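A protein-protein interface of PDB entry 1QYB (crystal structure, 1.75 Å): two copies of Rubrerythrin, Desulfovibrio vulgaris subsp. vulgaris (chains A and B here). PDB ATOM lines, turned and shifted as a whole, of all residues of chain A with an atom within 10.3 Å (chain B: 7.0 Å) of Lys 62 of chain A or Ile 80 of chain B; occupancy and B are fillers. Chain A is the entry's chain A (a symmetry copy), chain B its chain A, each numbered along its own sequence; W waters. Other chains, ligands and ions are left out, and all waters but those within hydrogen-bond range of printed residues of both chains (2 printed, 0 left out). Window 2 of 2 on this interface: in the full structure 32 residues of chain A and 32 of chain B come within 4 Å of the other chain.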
ATOM      1  N   LEU A   4      19.370  36.287  -9.250  1.00  0.00           N
ATOM      2  CA  LEU A   4      18.772  36.469  -7.932  1.00  0.00           C
ATOM      3  C   LEU A   4      19.835  36.805  -6.891  1.00  0.00           C
ATOM      4  O   LEU A   4      19.523  37.303  -5.811  1.00  0.00           O
ATOM      5  CB  LEU A   4      18.045  35.189  -7.511  1.00  0.00           C
ATOM      6  CG  LEU A   4      16.832  34.766  -8.339  1.00  0.00           C
ATOM      7  CD1 LEU A   4      16.483  33.316  -8.040  1.00  0.00           C
ATOM      8  CD2 LEU A   4      15.661  35.682  -8.020  1.00  0.00           C
ATOM      9  N   ILE A  13      13.205  32.921  -1.211  1.00  0.00           N
ATOM     10  CA  ILE A  13      12.965  31.639  -1.863  1.00  0.00           C
ATOM     11  C   ILE A  13      13.547  30.508  -1.014  1.00  0.00           C
ATOM     12  O   ILE A  13      12.897  29.486  -0.795  1.00  0.00           O
ATOM     13  CB  ILE A  13      13.605  31.586  -3.268  1.00  0.00           C
ATOM     14  CG1 ILE A  13      12.889  32.566  -4.200  1.00  0.00           C
ATOM     15  CG2 ILE A  13      13.523  30.165  -3.831  1.00  0.00           C
ATOM     16  CD1 ILE A  13      13.502  32.657  -5.583  1.00  0.00           C
ATOM     17  N   LEU A  14      14.773  30.685  -0.536  1.00  0.00           N
ATOM     18  CA  LEU A  14      15.382  29.646   0.283  1.00  0.00           C
ATOM     19  C   LEU A  14      14.606  29.483   1.590  1.00  0.00           C
ATOM     20  O   LEU A  14      14.419  28.368   2.070  1.00  0.00           O
ATOM     21  CB  LEU A  14      16.853  29.973   0.568  1.00  0.00           C
ATOM     22  CG  LEU A  14      17.628  28.940   1.400  1.00  0.00           C
ATOM     23  CD1 LEU A  14      17.514  27.558   0.767  1.00  0.00           C
ATOM     24  CD2 LEU A  14      19.089  29.359   1.500  1.00  0.00           C
ATOM     25  N   PHE A  17      11.616  27.545   0.875  1.00  0.00           N
ATOM     26  CA  PHE A  17      12.037  26.169   0.647  1.00  0.00           C
ATOM     27  C   PHE A  17      12.285  25.463   1.980  1.00  0.00           C
ATOM     28  O   PHE A  17      11.886  24.316   2.166  1.00  0.00           O
ATOM     29  CB  PHE A  17      13.312  26.133  -0.201  1.00  0.00           C
ATOM     30  CG  PHE A  17      13.829  24.744  -0.457  1.00  0.00           C
ATOM     31  CD1 PHE A  17      13.159  23.883  -1.321  1.00  0.00           C
ATOM     32  CD2 PHE A  17      14.978  24.289   0.182  1.00  0.00           C
ATOM     33  CE1 PHE A  17      13.629  22.582  -1.548  1.00  0.00           C
ATOM     34  CE2 PHE A  17      15.453  23.000  -0.036  1.00  0.00           C
ATOM     35  CZ  PHE A  17      14.777  22.141  -0.904  1.00  0.00           C
ATOM     36  N   ARG A  54       6.174  19.033  -1.101  1.00  0.00           N
ATOM     37  CA  ARG A  54       7.413  18.617  -1.764  1.00  0.00           C
ATOM     38  C   ARG A  54       7.479  19.303  -3.130  1.00  0.00           C
ATOM     39  O   ARG A  54       8.547  19.711  -3.578  1.00  0.00           O
ATOM     40  CB  ARG A  54       7.436  17.099  -1.968  1.00  0.00           C
ATOM     41  CG  ARG A  54       8.601  16.578  -2.828  1.00  0.00           C
ATOM     42  CD  ARG A  54       8.331  15.140  -3.280  1.00  0.00           C
ATOM     43  NE  ARG A  54       7.146  15.100  -4.133  1.00  0.00           N
ATOM     44  CZ  ARG A  54       6.326  14.061  -4.250  1.00  0.00           C
ATOM     45  NH1 ARG A  54       6.550  12.942  -3.570  1.00  0.00           N
ATOM     46  NH2 ARG A  54       5.259  14.156  -5.035  1.00  0.00           N
ATOM     47  N   GLU A  55       6.324  19.430  -3.780  1.00  0.00           N
ATOM     48  CA  GLU A  55       6.255  20.054  -5.098  1.00  0.00           C
ATOM     49  C   GLU A  55       6.398  21.582  -5.067  1.00  0.00           C
ATOM     50  O   GLU A  55       6.982  22.167  -5.981  1.00  0.00           O
ATOM     51  CB  GLU A  55       4.962  19.626  -5.797  1.00  0.00           C
ATOM     52  CG  GLU A  55       4.917  18.124  -6.083  1.00  0.00           C
ATOM     53  CD  GLU A  55       6.095  17.649  -6.929  1.00  0.00           C
ATOM     54  OE1 GLU A  55       6.380  18.287  -7.960  1.00  0.00           O
ATOM     55  OE2 GLU A  55       6.729  16.631  -6.569  1.00  0.00           O
ATOM     56  N   HIS A  56       5.869  22.228  -4.030  1.00  0.00           N
ATOM     57  CA  HIS A  56       6.026  23.680  -3.888  1.00  0.00           C
ATOM     58  C   HIS A  56       7.529  23.913  -3.714  1.00  0.00           C
ATOM     59  O   HIS A  56       8.124  24.773  -4.362  1.00  0.00           O
ATOM     60  CB  HIS A  56       5.330  24.195  -2.625  1.00  0.00           C
ATOM     61  CG  HIS A  56       3.840  24.065  -2.645  1.00  0.00           C
ATOM     62  ND1 HIS A  56       3.073  24.193  -1.506  1.00  0.00           N
ATOM     63  CD2 HIS A  56       2.975  23.837  -3.660  1.00  0.00           C
ATOM     64  CE1 HIS A  56       1.799  24.045  -1.819  1.00  0.00           C
ATOM     65  NE2 HIS A  56       1.711  23.829  -3.119  1.00  0.00           N
ATOM     66  N   ALA A  57       8.129  23.134  -2.817  1.00  0.00           N
ATOM     67  CA  ALA A  57       9.556  23.234  -2.538  1.00  0.00           C
ATOM     68  C   ALA A  57      10.401  23.016  -3.794  1.00  0.00           C
ATOM     69  O   ALA A  57      11.410  23.696  -3.993  1.00  0.00           O
ATOM     70  CB  ALA A  57       9.946  22.217  -1.468  1.00  0.00           C
ATOM     71  N   LYS A  58       9.995  22.064  -4.630  1.00  0.00           N
ATOM     72  CA  LYS A  58      10.729  21.755  -5.856  1.00  0.00           C
ATOM     73  C   LYS A  58      10.724  22.941  -6.816  1.00  0.00           C
ATOM     74  O   LYS A  58      11.763  23.292  -7.383  1.00  0.00           O
ATOM     75  CB  LYS A  58      10.125  20.528  -6.544  1.00  0.00           C
ATOM     76  CG  LYS A  58      10.916  20.033  -7.746  1.00  0.00           C
ATOM     77  CD  LYS A  58      10.244  18.819  -8.375  1.00  0.00           C
ATOM     78  CE  LYS A  58      11.019  18.321  -9.587  1.00  0.00           C
ATOM     79  NZ  LYS A  58      10.421  17.075 -10.147  1.00  0.00           N
ATOM     80  N   ARG A  59       9.558  23.553  -7.000  1.00  0.00           N
ATOM     81  CA  ARG A  59       9.438  24.710  -7.878  1.00  0.00           C
ATOM     82  C   ARG A  59      10.341  25.826  -7.360  1.00  0.00           C
ATOM     83  O   ARG A  59      11.052  26.474  -8.134  1.00  0.00           O
ATOM     84  CB  ARG A  59       7.981  25.202  -7.926  1.00  0.00           C
ATOM     85  CG  ARG A  59       7.735  26.343  -8.926  1.00  0.00           C
ATOM     86  CD  ARG A  59       7.937  25.871 -10.363  1.00  0.00           C
ATOM     87  NE  ARG A  59       8.036  26.967 -11.330  1.00  0.00           N
ATOM     88  CZ  ARG A  59       7.011  27.689 -11.774  1.00  0.00           C
ATOM     89  NH1 ARG A  59       5.779  27.449 -11.346  1.00  0.00           N
ATOM     90  NH2 ARG A  59       7.220  28.653 -12.661  1.00  0.00           N
ATOM     91  N   LEU A  60      10.318  26.038  -6.048  1.00  0.00           N
ATOM     92  CA  LEU A  60      11.126  27.082  -5.427  1.00  0.00           C
ATOM     93  C   LEU A  60      12.609  26.782  -5.569  1.00  0.00           C
ATOM     94  O   LEU A  60      13.394  27.654  -5.936  1.00  0.00           O
ATOM     95  CB  LEU A  60      10.772  27.217  -3.941  1.00  0.00           C
ATOM     96  CG  LEU A  60       9.354  27.675  -3.600  1.00  0.00           C
ATOM     97  CD1 LEU A  60       9.083  27.463  -2.113  1.00  0.00           C
ATOM     98  CD2 LEU A  60       9.189  29.140  -3.985  1.00  0.00           C
ATOM     99  N   PHE A  61      12.978  25.536  -5.285  1.00  0.00           N
ATOM    100  CA  PHE A  61      14.366  25.093  -5.355  1.00  0.00           C
ATOM    101  C   PHE A  61      14.987  25.288  -6.735  1.00  0.00           C
ATOM    102  O   PHE A  61      16.158  25.652  -6.854  1.00  0.00           O
ATOM    103  CB  PHE A  61      14.455  23.616  -4.969  1.00  0.00           C
ATOM    104  CG  PHE A  61      15.855  23.128  -4.728  1.00  0.00           C
ATOM    105  CD1 PHE A  61      16.550  23.502  -3.581  1.00  0.00           C
ATOM    106  CD2 PHE A  61      16.471  22.269  -5.632  1.00  0.00           C
ATOM    107  CE1 PHE A  61      17.836  23.021  -3.334  1.00  0.00           C
ATOM    108  CE2 PHE A  61      17.758  21.781  -5.394  1.00  0.00           C
ATOM    109  CZ  PHE A  61      18.439  22.157  -4.243  1.00  0.00           C
ATOM    110  N   LYS A  62      14.203  25.039  -7.777  1.00  0.00           N
ATOM    111  CA  LYS A  62      14.698  25.165  -9.135  1.00  0.00           C
ATOM    112  C   LYS A  62      14.981  26.601  -9.577  1.00  0.00           C
ATOM    113  O   LYS A  62      15.575  26.814 -10.633  1.00  0.00           O
ATOM    114  CB  LYS A  62      13.732  24.469 -10.102  1.00  0.00           C
ATOM    115  CG  LYS A  62      13.790  22.937  -9.982  1.00  0.00           C
ATOM    116  CD  LYS A  62      12.748  22.228 -10.841  1.00  0.00           C
ATOM    117  CE  LYS A  62      13.027  22.387 -12.327  1.00  0.00           C
ATOM    118  NZ  LYS A  62      12.066  21.599 -13.151  1.00  0.00           N
ATOM    119  N   PHE A  63      14.572  27.578  -8.772  1.00  0.00           N
ATOM    120  CA  PHE A  63      14.828  28.980  -9.103  1.00  0.00           C
ATOM    121  C   PHE A  63      16.208  29.416  -8.616  1.00  0.00           C
ATOM    122  O   PHE A  63      16.779  30.378  -9.131  1.00  0.00           O
ATOM    123  CB  PHE A  63      13.780  29.902  -8.466  1.00  0.00           C
ATOM    124  CG  PHE A  63      12.502  30.016  -9.248  1.00  0.00           C
ATOM    125  CD1 PHE A  63      12.523  30.346 -10.599  1.00  0.00           C
ATOM    126  CD2 PHE A  63      11.271  29.832  -8.625  1.00  0.00           C
ATOM    127  CE1 PHE A  63      11.340  30.492 -11.319  1.00  0.00           C
ATOM    128  CE2 PHE A  63      10.079  29.977  -9.338  1.00  0.00           C
ATOM    129  CZ  PHE A  63      10.115  30.307 -10.687  1.00  0.00           C
ATOM    130  N   LEU A  64      16.739  28.708  -7.623  1.00  0.00           N
ATOM    131  CA  LEU A  64      18.033  29.054  -7.047  1.00  0.00           C
ATOM    132  C   LEU A  64      19.210  28.829  -7.988  1.00  0.00           C
ATOM    133  O   LEU A  64      19.177  27.953  -8.853  1.00  0.00           O
ATOM    134  CB  LEU A  64      18.224  28.299  -5.731  1.00  0.00           C
ATOM    135  CG  LEU A  64      17.113  28.643  -4.728  1.00  0.00           C
ATOM    136  CD1 LEU A  64      17.281  27.834  -3.453  1.00  0.00           C
ATOM    137  CD2 LEU A  64      17.143  30.134  -4.427  1.00  0.00           C
ATOM    138  N   GLU A  65      20.255  29.631  -7.805  1.00  0.00           N
ATOM    139  CA  GLU A  65      21.427  29.569  -8.670  1.00  0.00           C
ATOM    140  C   GLU A  65      22.665  28.903  -8.079  1.00  0.00           C
ATOM    141  O   GLU A  65      23.732  28.933  -8.690  1.00  0.00           O
ATOM    142  CB  GLU A  65      21.785  30.983  -9.135  1.00  0.00           C
ATOM    143  CG  GLU A  65      20.572  31.822  -9.512  1.00  0.00           C
ATOM    144  CD  GLU A  65      20.945  33.195 -10.036  1.00  0.00           C
ATOM    145  OE1 GLU A  65      21.832  33.842  -9.439  1.00  0.00           O
ATOM    146  OE2 GLU A  65      20.342  33.632 -11.039  1.00  0.00           O
ATOM    147  N   GLY A  66      22.532  28.311  -6.897  1.00  0.00           N
ATOM    148  CA  GLY A  66      23.670  27.640  -6.292  1.00  0.00           C
ATOM    149  C   GLY A  66      24.355  28.397  -5.169  1.00  0.00           C
ATOM    150  O   GLY A  66      24.047  29.559  -4.905  1.00  0.00           O
ATOM    151  N   GLY A  67      25.294  27.727  -4.509  1.00  0.00           N
ATOM    152  CA  GLY A  67      26.022  28.340  -3.413  1.00  0.00           C
ATOM    153  C   GLY A  67      25.291  28.212  -2.091  1.00  0.00           C
ATOM    154  O   GLY A  67      24.095  27.926  -2.061  1.00  0.00           O
ATOM    155  N   GLU A 116       7.984  36.668 -12.680  1.00  0.00           N
ATOM    156  CA  GLU A 116       7.621  35.254 -12.727  1.00  0.00           C
ATOM    157  C   GLU A 116       7.591  34.645 -11.332  1.00  0.00           C
ATOM    158  O   GLU A 116       6.643  33.947 -10.969  1.00  0.00           O
ATOM    159  CB  GLU A 116       8.605  34.464 -13.591  1.00  0.00           C
ATOM    160  CG  GLU A 116       8.255  32.980 -13.698  1.00  0.00           C
ATOM    161  CD  GLU A 116       9.317  32.161 -14.415  1.00  0.00           C
ATOM    162  OE1 GLU A 116       9.088  30.951 -14.630  1.00  0.00           O
ATOM    163  OE2 GLU A 116      10.380  32.721 -14.761  1.00  0.00           O
ATOM    164  N   ILE A 117       8.638  34.909 -10.556  1.00  0.00           N
ATOM    165  CA  ILE A 117       8.743  34.379  -9.204  1.00  0.00           C
ATOM    166  C   ILE A 117       7.650  34.923  -8.291  1.00  0.00           C
ATOM    167  O   ILE A 117       7.086  34.188  -7.477  1.00  0.00           O
ATOM    168  CB  ILE A 117      10.129  34.692  -8.603  1.00  0.00           C
ATOM    169  CG1 ILE A 117      11.201  33.912  -9.369  1.00  0.00           C
ATOM    170  CG2 ILE A 117      10.156  34.343  -7.127  1.00  0.00           C
ATOM    171  CD1 ILE A 117      12.613  34.156  -8.891  1.00  0.00           C
ATOM    172  N   VAL A 120       4.590  33.095  -8.900  1.00  0.00           N
ATOM    173  CA  VAL A 120       4.649  31.734  -8.380  1.00  0.00           C
ATOM    174  C   VAL A 120       4.336  31.770  -6.885  1.00  0.00           C
ATOM    175  O   VAL A 120       3.614  30.911  -6.380  1.00  0.00           O
ATOM    176  CB  VAL A 120       6.038  31.093  -8.616  1.00  0.00           C
ATOM    177  CG1 VAL A 120       6.140  29.766  -7.874  1.00  0.00           C
ATOM    178  CG2 VAL A 120       6.247  30.867 -10.106  1.00  0.00           C
ATOM    179  N   ILE A 124       1.268  29.747  -5.176  1.00  0.00           N
ATOM    180  CA  ILE A 124       1.449  28.783  -4.099  1.00  0.00           C
ATOM    181  C   ILE A 124       0.519  29.136  -2.946  1.00  0.00           C
ATOM    182  O   ILE A 124      -0.037  28.255  -2.302  1.00  0.00           O
ATOM    183  CB  ILE A 124       2.917  28.758  -3.599  1.00  0.00           C
ATOM    184  CG1 ILE A 124       3.820  28.176  -4.693  1.00  0.00           C
ATOM    185  CG2 ILE A 124       3.027  27.942  -2.317  1.00  0.00           C
ATOM    186  CD1 ILE A 124       5.302  28.123  -4.323  1.00  0.00           C
ATOM    187  N   ARG B  26      15.955  17.529  -1.454  1.00  0.00           N
ATOM    188  CA  ARG B  26      17.034  17.503  -2.438  1.00  0.00           C
ATOM    189  C   ARG B  26      17.302  16.084  -2.938  1.00  0.00           C
ATOM    190  O   ARG B  26      17.417  15.861  -4.143  1.00  0.00           O
ATOM    191  CB  ARG B  26      18.333  18.097  -1.857  1.00  0.00           C
ATOM    192  CG  ARG B  26      18.289  19.599  -1.552  1.00  0.00           C
ATOM    193  CD  ARG B  26      19.705  20.179  -1.415  1.00  0.00           C
ATOM    194  NE  ARG B  26      20.522  19.441  -0.448  1.00  0.00           N
ATOM    195  CZ  ARG B  26      20.505  19.642   0.868  1.00  0.00           C
ATOM    196  NH1 ARG B  26      19.716  20.568   1.392  1.00  0.00           N
ATOM    197  NH2 ARG B  26      21.269  18.905   1.664  1.00  0.00           N
ATOM    198  N   TYR B  29      14.715  14.847  -5.304  1.00  0.00           N
ATOM    199  CA  TYR B  29      14.837  15.486  -6.607  1.00  0.00           C
ATOM    200  C   TYR B  29      15.983  14.857  -7.383  1.00  0.00           C
ATOM    201  O   TYR B  29      15.852  14.602  -8.577  1.00  0.00           O
ATOM    202  CB  TYR B  29      15.081  16.995  -6.484  1.00  0.00           C
ATOM    203  CG  TYR B  29      14.085  17.739  -5.623  1.00  0.00           C
ATOM    204  CD1 TYR B  29      12.779  17.274  -5.457  1.00  0.00           C
ATOM    205  CD2 TYR B  29      14.457  18.909  -4.963  1.00  0.00           C
ATOM    206  CE1 TYR B  29      11.869  17.957  -4.642  1.00  0.00           C
ATOM    207  CE2 TYR B  29      13.559  19.601  -4.155  1.00  0.00           C
ATOM    208  CZ  TYR B  29      12.270  19.119  -3.997  1.00  0.00           C
ATOM    209  OH  TYR B  29      11.394  19.807  -3.186  1.00  0.00           O
ATOM    210  N   PHE B  30      17.101  14.605  -6.706  1.00  0.00           N
ATOM    211  CA  PHE B  30      18.253  13.997  -7.368  1.00  0.00           C
ATOM    212  C   PHE B  30      17.888  12.580  -7.791  1.00  0.00           C
ATOM    213  O   PHE B  30      18.413  12.059  -8.773  1.00  0.00           O
ATOM    214  CB  PHE B  30      19.471  13.942  -6.433  1.00  0.00           C
ATOM    215  CG  PHE B  30      19.976  15.296  -5.992  1.00  0.00           C
ATOM    216  CD1 PHE B  30      19.727  16.440  -6.747  1.00  0.00           C
ATOM    217  CD2 PHE B  30      20.740  15.414  -4.833  1.00  0.00           C
ATOM    218  CE1 PHE B  30      20.230  17.682  -6.354  1.00  0.00           C
ATOM    219  CE2 PHE B  30      21.249  16.645  -4.430  1.00  0.00           C
ATOM    220  CZ  PHE B  30      20.994  17.784  -5.190  1.00  0.00           C
ATOM    221  N   GLN B  33      16.198  12.830 -11.051  1.00  0.00           N
ATOM    222  CA  GLN B  33      17.155  13.147 -12.108  1.00  0.00           C
ATOM    223  C   GLN B  33      17.965  11.905 -12.490  1.00  0.00           C
ATOM    224  O   GLN B  33      18.289  11.699 -13.663  1.00  0.00           O
ATOM    225  CB  GLN B  33      18.090  14.272 -11.653  1.00  0.00           C
ATOM    226  CG  GLN B  33      19.009  14.784 -12.751  1.00  0.00           C
ATOM    227  CD  GLN B  33      18.235  15.288 -13.958  1.00  0.00           C
ATOM    228  OE1 GLN B  33      17.331  16.115 -13.829  1.00  0.00           O
ATOM    229  NE2 GLN B  33      18.586  14.792 -15.137  1.00  0.00           N
ATOM    230  N   LYS B  36      16.013   9.918 -14.907  1.00  0.00           N
ATOM    231  CA  LYS B  36      16.099  10.522 -16.232  1.00  0.00           C
ATOM    232  C   LYS B  36      17.451  10.238 -16.873  1.00  0.00           C
ATOM    233  O   LYS B  36      17.538  10.041 -18.086  1.00  0.00           O
ATOM    234  CB  LYS B  36      15.879  12.035 -16.151  1.00  0.00           C
ATOM    235  CG  LYS B  36      14.499  12.439 -15.649  1.00  0.00           C
ATOM    236  CD  LYS B  36      14.383  13.954 -15.513  1.00  0.00           C
ATOM    237  CE  LYS B  36      13.030  14.358 -14.946  1.00  0.00           C
ATOM    238  NZ  LYS B  36      12.949  15.825 -14.695  1.00  0.00           N
ATOM    239  N   GLY B  78      19.986  25.564  -4.051  1.00  0.00           N
ATOM    240  CA  GLY B  78      20.048  24.869  -5.327  1.00  0.00           C
ATOM    241  C   GLY B  78      21.205  23.889  -5.217  1.00  0.00           C
ATOM    242  O   GLY B  78      21.829  23.818  -4.155  1.00  0.00           O
ATOM    243  N   ILE B  79      21.501  23.119  -6.263  1.00  0.00           N
ATOM    244  CA  ILE B  79      20.777  23.138  -7.531  1.00  0.00           C
ATOM    245  C   ILE B  79      20.661  21.691  -7.996  1.00  0.00           C
ATOM    246  O   ILE B  79      21.257  20.793  -7.401  1.00  0.00           O
ATOM    247  CB  ILE B  79      21.550  23.909  -8.629  1.00  0.00           C
ATOM    248  CG1 ILE B  79      22.867  23.187  -8.944  1.00  0.00           C
ATOM    249  CG2 ILE B  79      21.819  25.330  -8.183  1.00  0.00           C
ATOM    250  CD1 ILE B  79      23.631  23.777 -10.109  1.00  0.00           C
ATOM    251  N   ILE B  80      19.891  21.469  -9.055  1.00  0.00           N
ATOM    252  CA  ILE B  80      19.736  20.132  -9.613  1.00  0.00           C
ATOM    253  C   ILE B  80      20.564  20.078 -10.893  1.00  0.00           C
ATOM    254  O   ILE B  80      20.261  20.779 -11.861  1.00  0.00           O
ATOM    255  CB  ILE B  80      18.267  19.821  -9.973  1.00  0.00           C
ATOM    256  CG1 ILE B  80      17.389  19.922  -8.724  1.00  0.00           C
ATOM    257  CG2 ILE B  80      18.168  18.423 -10.585  1.00  0.00           C
ATOM    258  CD1 ILE B  80      15.904  19.736  -8.999  1.00  0.00           C
ATOM    259  N   ALA B  81      21.611  19.258 -10.892  1.00  0.00           N
ATOM    260  CA  ALA B  81      22.476  19.112 -12.061  1.00  0.00           C
ATOM    261  C   ALA B  81      22.438  17.661 -12.537  1.00  0.00           C
ATOM    262  O   ALA B  81      21.478  16.943 -12.262  1.00  0.00           O
ATOM    263  CB  ALA B  81      23.906  19.510 -11.701  1.00  0.00           C
ATOM    264  N   ASP B  82      23.468  17.239 -13.267  1.00  0.00           N
ATOM    265  CA  ASP B  82      23.551  15.860 -13.740  1.00  0.00           C
ATOM    266  C   ASP B  82      23.771  14.979 -12.513  1.00  0.00           C
ATOM    267  O   ASP B  82      24.201  15.465 -11.469  1.00  0.00           O
ATOM    268  CB  ASP B  82      24.733  15.690 -14.688  1.00  0.00           C
ATOM    269  CG  ASP B  82      26.023  16.203 -14.088  1.00  0.00           C
ATOM    270  OD1 ASP B  82      26.182  17.442 -14.001  1.00  0.00           O
ATOM    271  OD2 ASP B  82      26.869  15.380 -13.688  1.00  0.00           O
ATOM    272  N   ALA B  85      27.220  15.132 -10.675  1.00  0.00           N
ATOM    273  CA  ALA B  85      27.347  16.346  -9.884  1.00  0.00           C
ATOM    274  C   ALA B  85      26.483  16.276  -8.627  1.00  0.00           C
ATOM    275  O   ALA B  85      26.909  16.701  -7.552  1.00  0.00           O
ATOM    276  CB  ALA B  85      26.959  17.556 -10.716  1.00  0.00           C
ATOM    277  N   ASN B  86      25.274  15.734  -8.758  1.00  0.00           N
ATOM    278  CA  ASN B  86      24.374  15.626  -7.614  1.00  0.00           C
ATOM    279  C   ASN B  86      24.955  14.700  -6.546  1.00  0.00           C
ATOM    280  O   ASN B  86      24.821  14.965  -5.350  1.00  0.00           O
ATOM    281  CB  ASN B  86      22.989  15.130  -8.060  1.00  0.00           C
ATOM    282  CG  ASN B  86      22.305  16.094  -9.014  1.00  0.00           C
ATOM    283  OD1 ASN B  86      22.571  17.297  -8.988  1.00  0.00           O
ATOM    284  ND2 ASN B  86      21.407  15.577  -9.848  1.00  0.00           N
HETATM  285  O   HOH W   1      11.259  16.642 -12.815  1.00  0.00           O
HETATM  286  O   HOH W   2      24.352  24.916  -3.897  1.00  0.00           O
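Of the 12 printed residues of chain B, 5 touch a printed residue of chain A.
Printed residues of chain B that touch a printed residue of chain A: Arg 26, Tyr 29, Gly 78, Ile 79 and Ile 80.
Hydrophobic or aromatic side chains of chain B that line the printed part of chain A: Tyr 29, Ile 79 and Ile 80.
Along chain B the printed residues that touch a printed residue of chain A span positions 26 to 80.
Printed residues of chain A that touch a printed residue of chain B: Phe 17, Arg 54, Ala 57, Lys 58, Phe 61, Lys 62, Leu 64, Glu 65 and Gly 66.
Among the printed residues, no Asp or Glu carboxylate lies within 4 Å of a Lys or Arg side-chain nitrogen of the other chain.
Water W1 bridges the side-chain amino group of Lys 36 of chain B (2.7 Å) and the side-chain amino group of Lys 58 of chain A (2.8 Å).
Water W2 bridges the backbone carbonyl oxygen (O) of Gly 78 of chain B (2.8 Å) and the backbone NH (N) of Gly 67 of chain A (3.0 Å).
The side-chain carboxylate of Glu 65 of chain A lies within hydrogen-bond range of the backbone NH of Leu 4 of chain A, 3.3 Å away.
The guanidinium group (NE) of Arg 54 of chain A is in salt-bridge range of the side-chain carboxylate (OE2) of Glu 55 of chain A (2.9 Å).
The side-chain hydroxyl of Tyr 29 of chain B sits at hydrogen-bond distance from the backbone carbonyl oxygen of Arg 54 of chain A.
The side-chain hydroxyl of Tyr 29 of chain B is in hydrogen-bond range of the backbone NH of Lys 58 of chain A, at 3.0 Å.
Lys 62 of chain A touches just one residue of chain B: Ile 80.
Of chain A, only Phe 61 and Lys 62 come within 4 Å of Ile 80 of chain B.
Of the printed residues of chain B, Lys 58 of chain A touches Tyr 29 (3.0 Å).
Printed residues of chain B within 4 Å of Phe 17 of chain A: Tyr 29 (3.9 Å).
Of the printed residues of chain B, Gly 66 of chain A touches Ile 79.
Printed residues of chain B within 4 Å of Phe 61 of chain A: Arg 26, Tyr 29, Gly 78, Ile 79 and Ile 80.
Ala 85 of chain B touches none of the printed residues of chain A.
The nearest printed residue of chain B that does not touch Lys 58 of chain A is Ile 80 of chain B (5.1 Å).
No position is printed for both chains.
Of the 14 pairs that touch across the chains among the printed residues, none has its exchanged pair printed and touching as well.
Among the printed residues, merely in contact across the chains: Ala 57 of chain A with Tyr 29 of chain B (3.3 Å), Gly 66 of chain A with Ile 79 of chain B (3.3 Å), Phe 61 of chain A with Gly 78 of chain B (3.3 Å), Leu 64 of chain A with Gly 78 of chain B (3.6 Å), Glu 65 of chain A with Ile 79 of chain B (3.7 Å), Phe 61 of chain A with Arg 26 of chain B (3.7 Å), Leu 64 of chain A with Ile 79 of chain B (3.8 Å), Phe 61 of chain A with Ile 79 of chain B (3.8 Å), Phe 61 of chain A with Ile 80 of chain B (3.8 Å), Phe 17 of chain A with Tyr 29 of chain B (3.9 Å), Lys 62 of chain A with Ile 80 of chain B (3.96 Å) and Phe 61 of chain A with Tyr 29 of chain B (3.97 Å).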
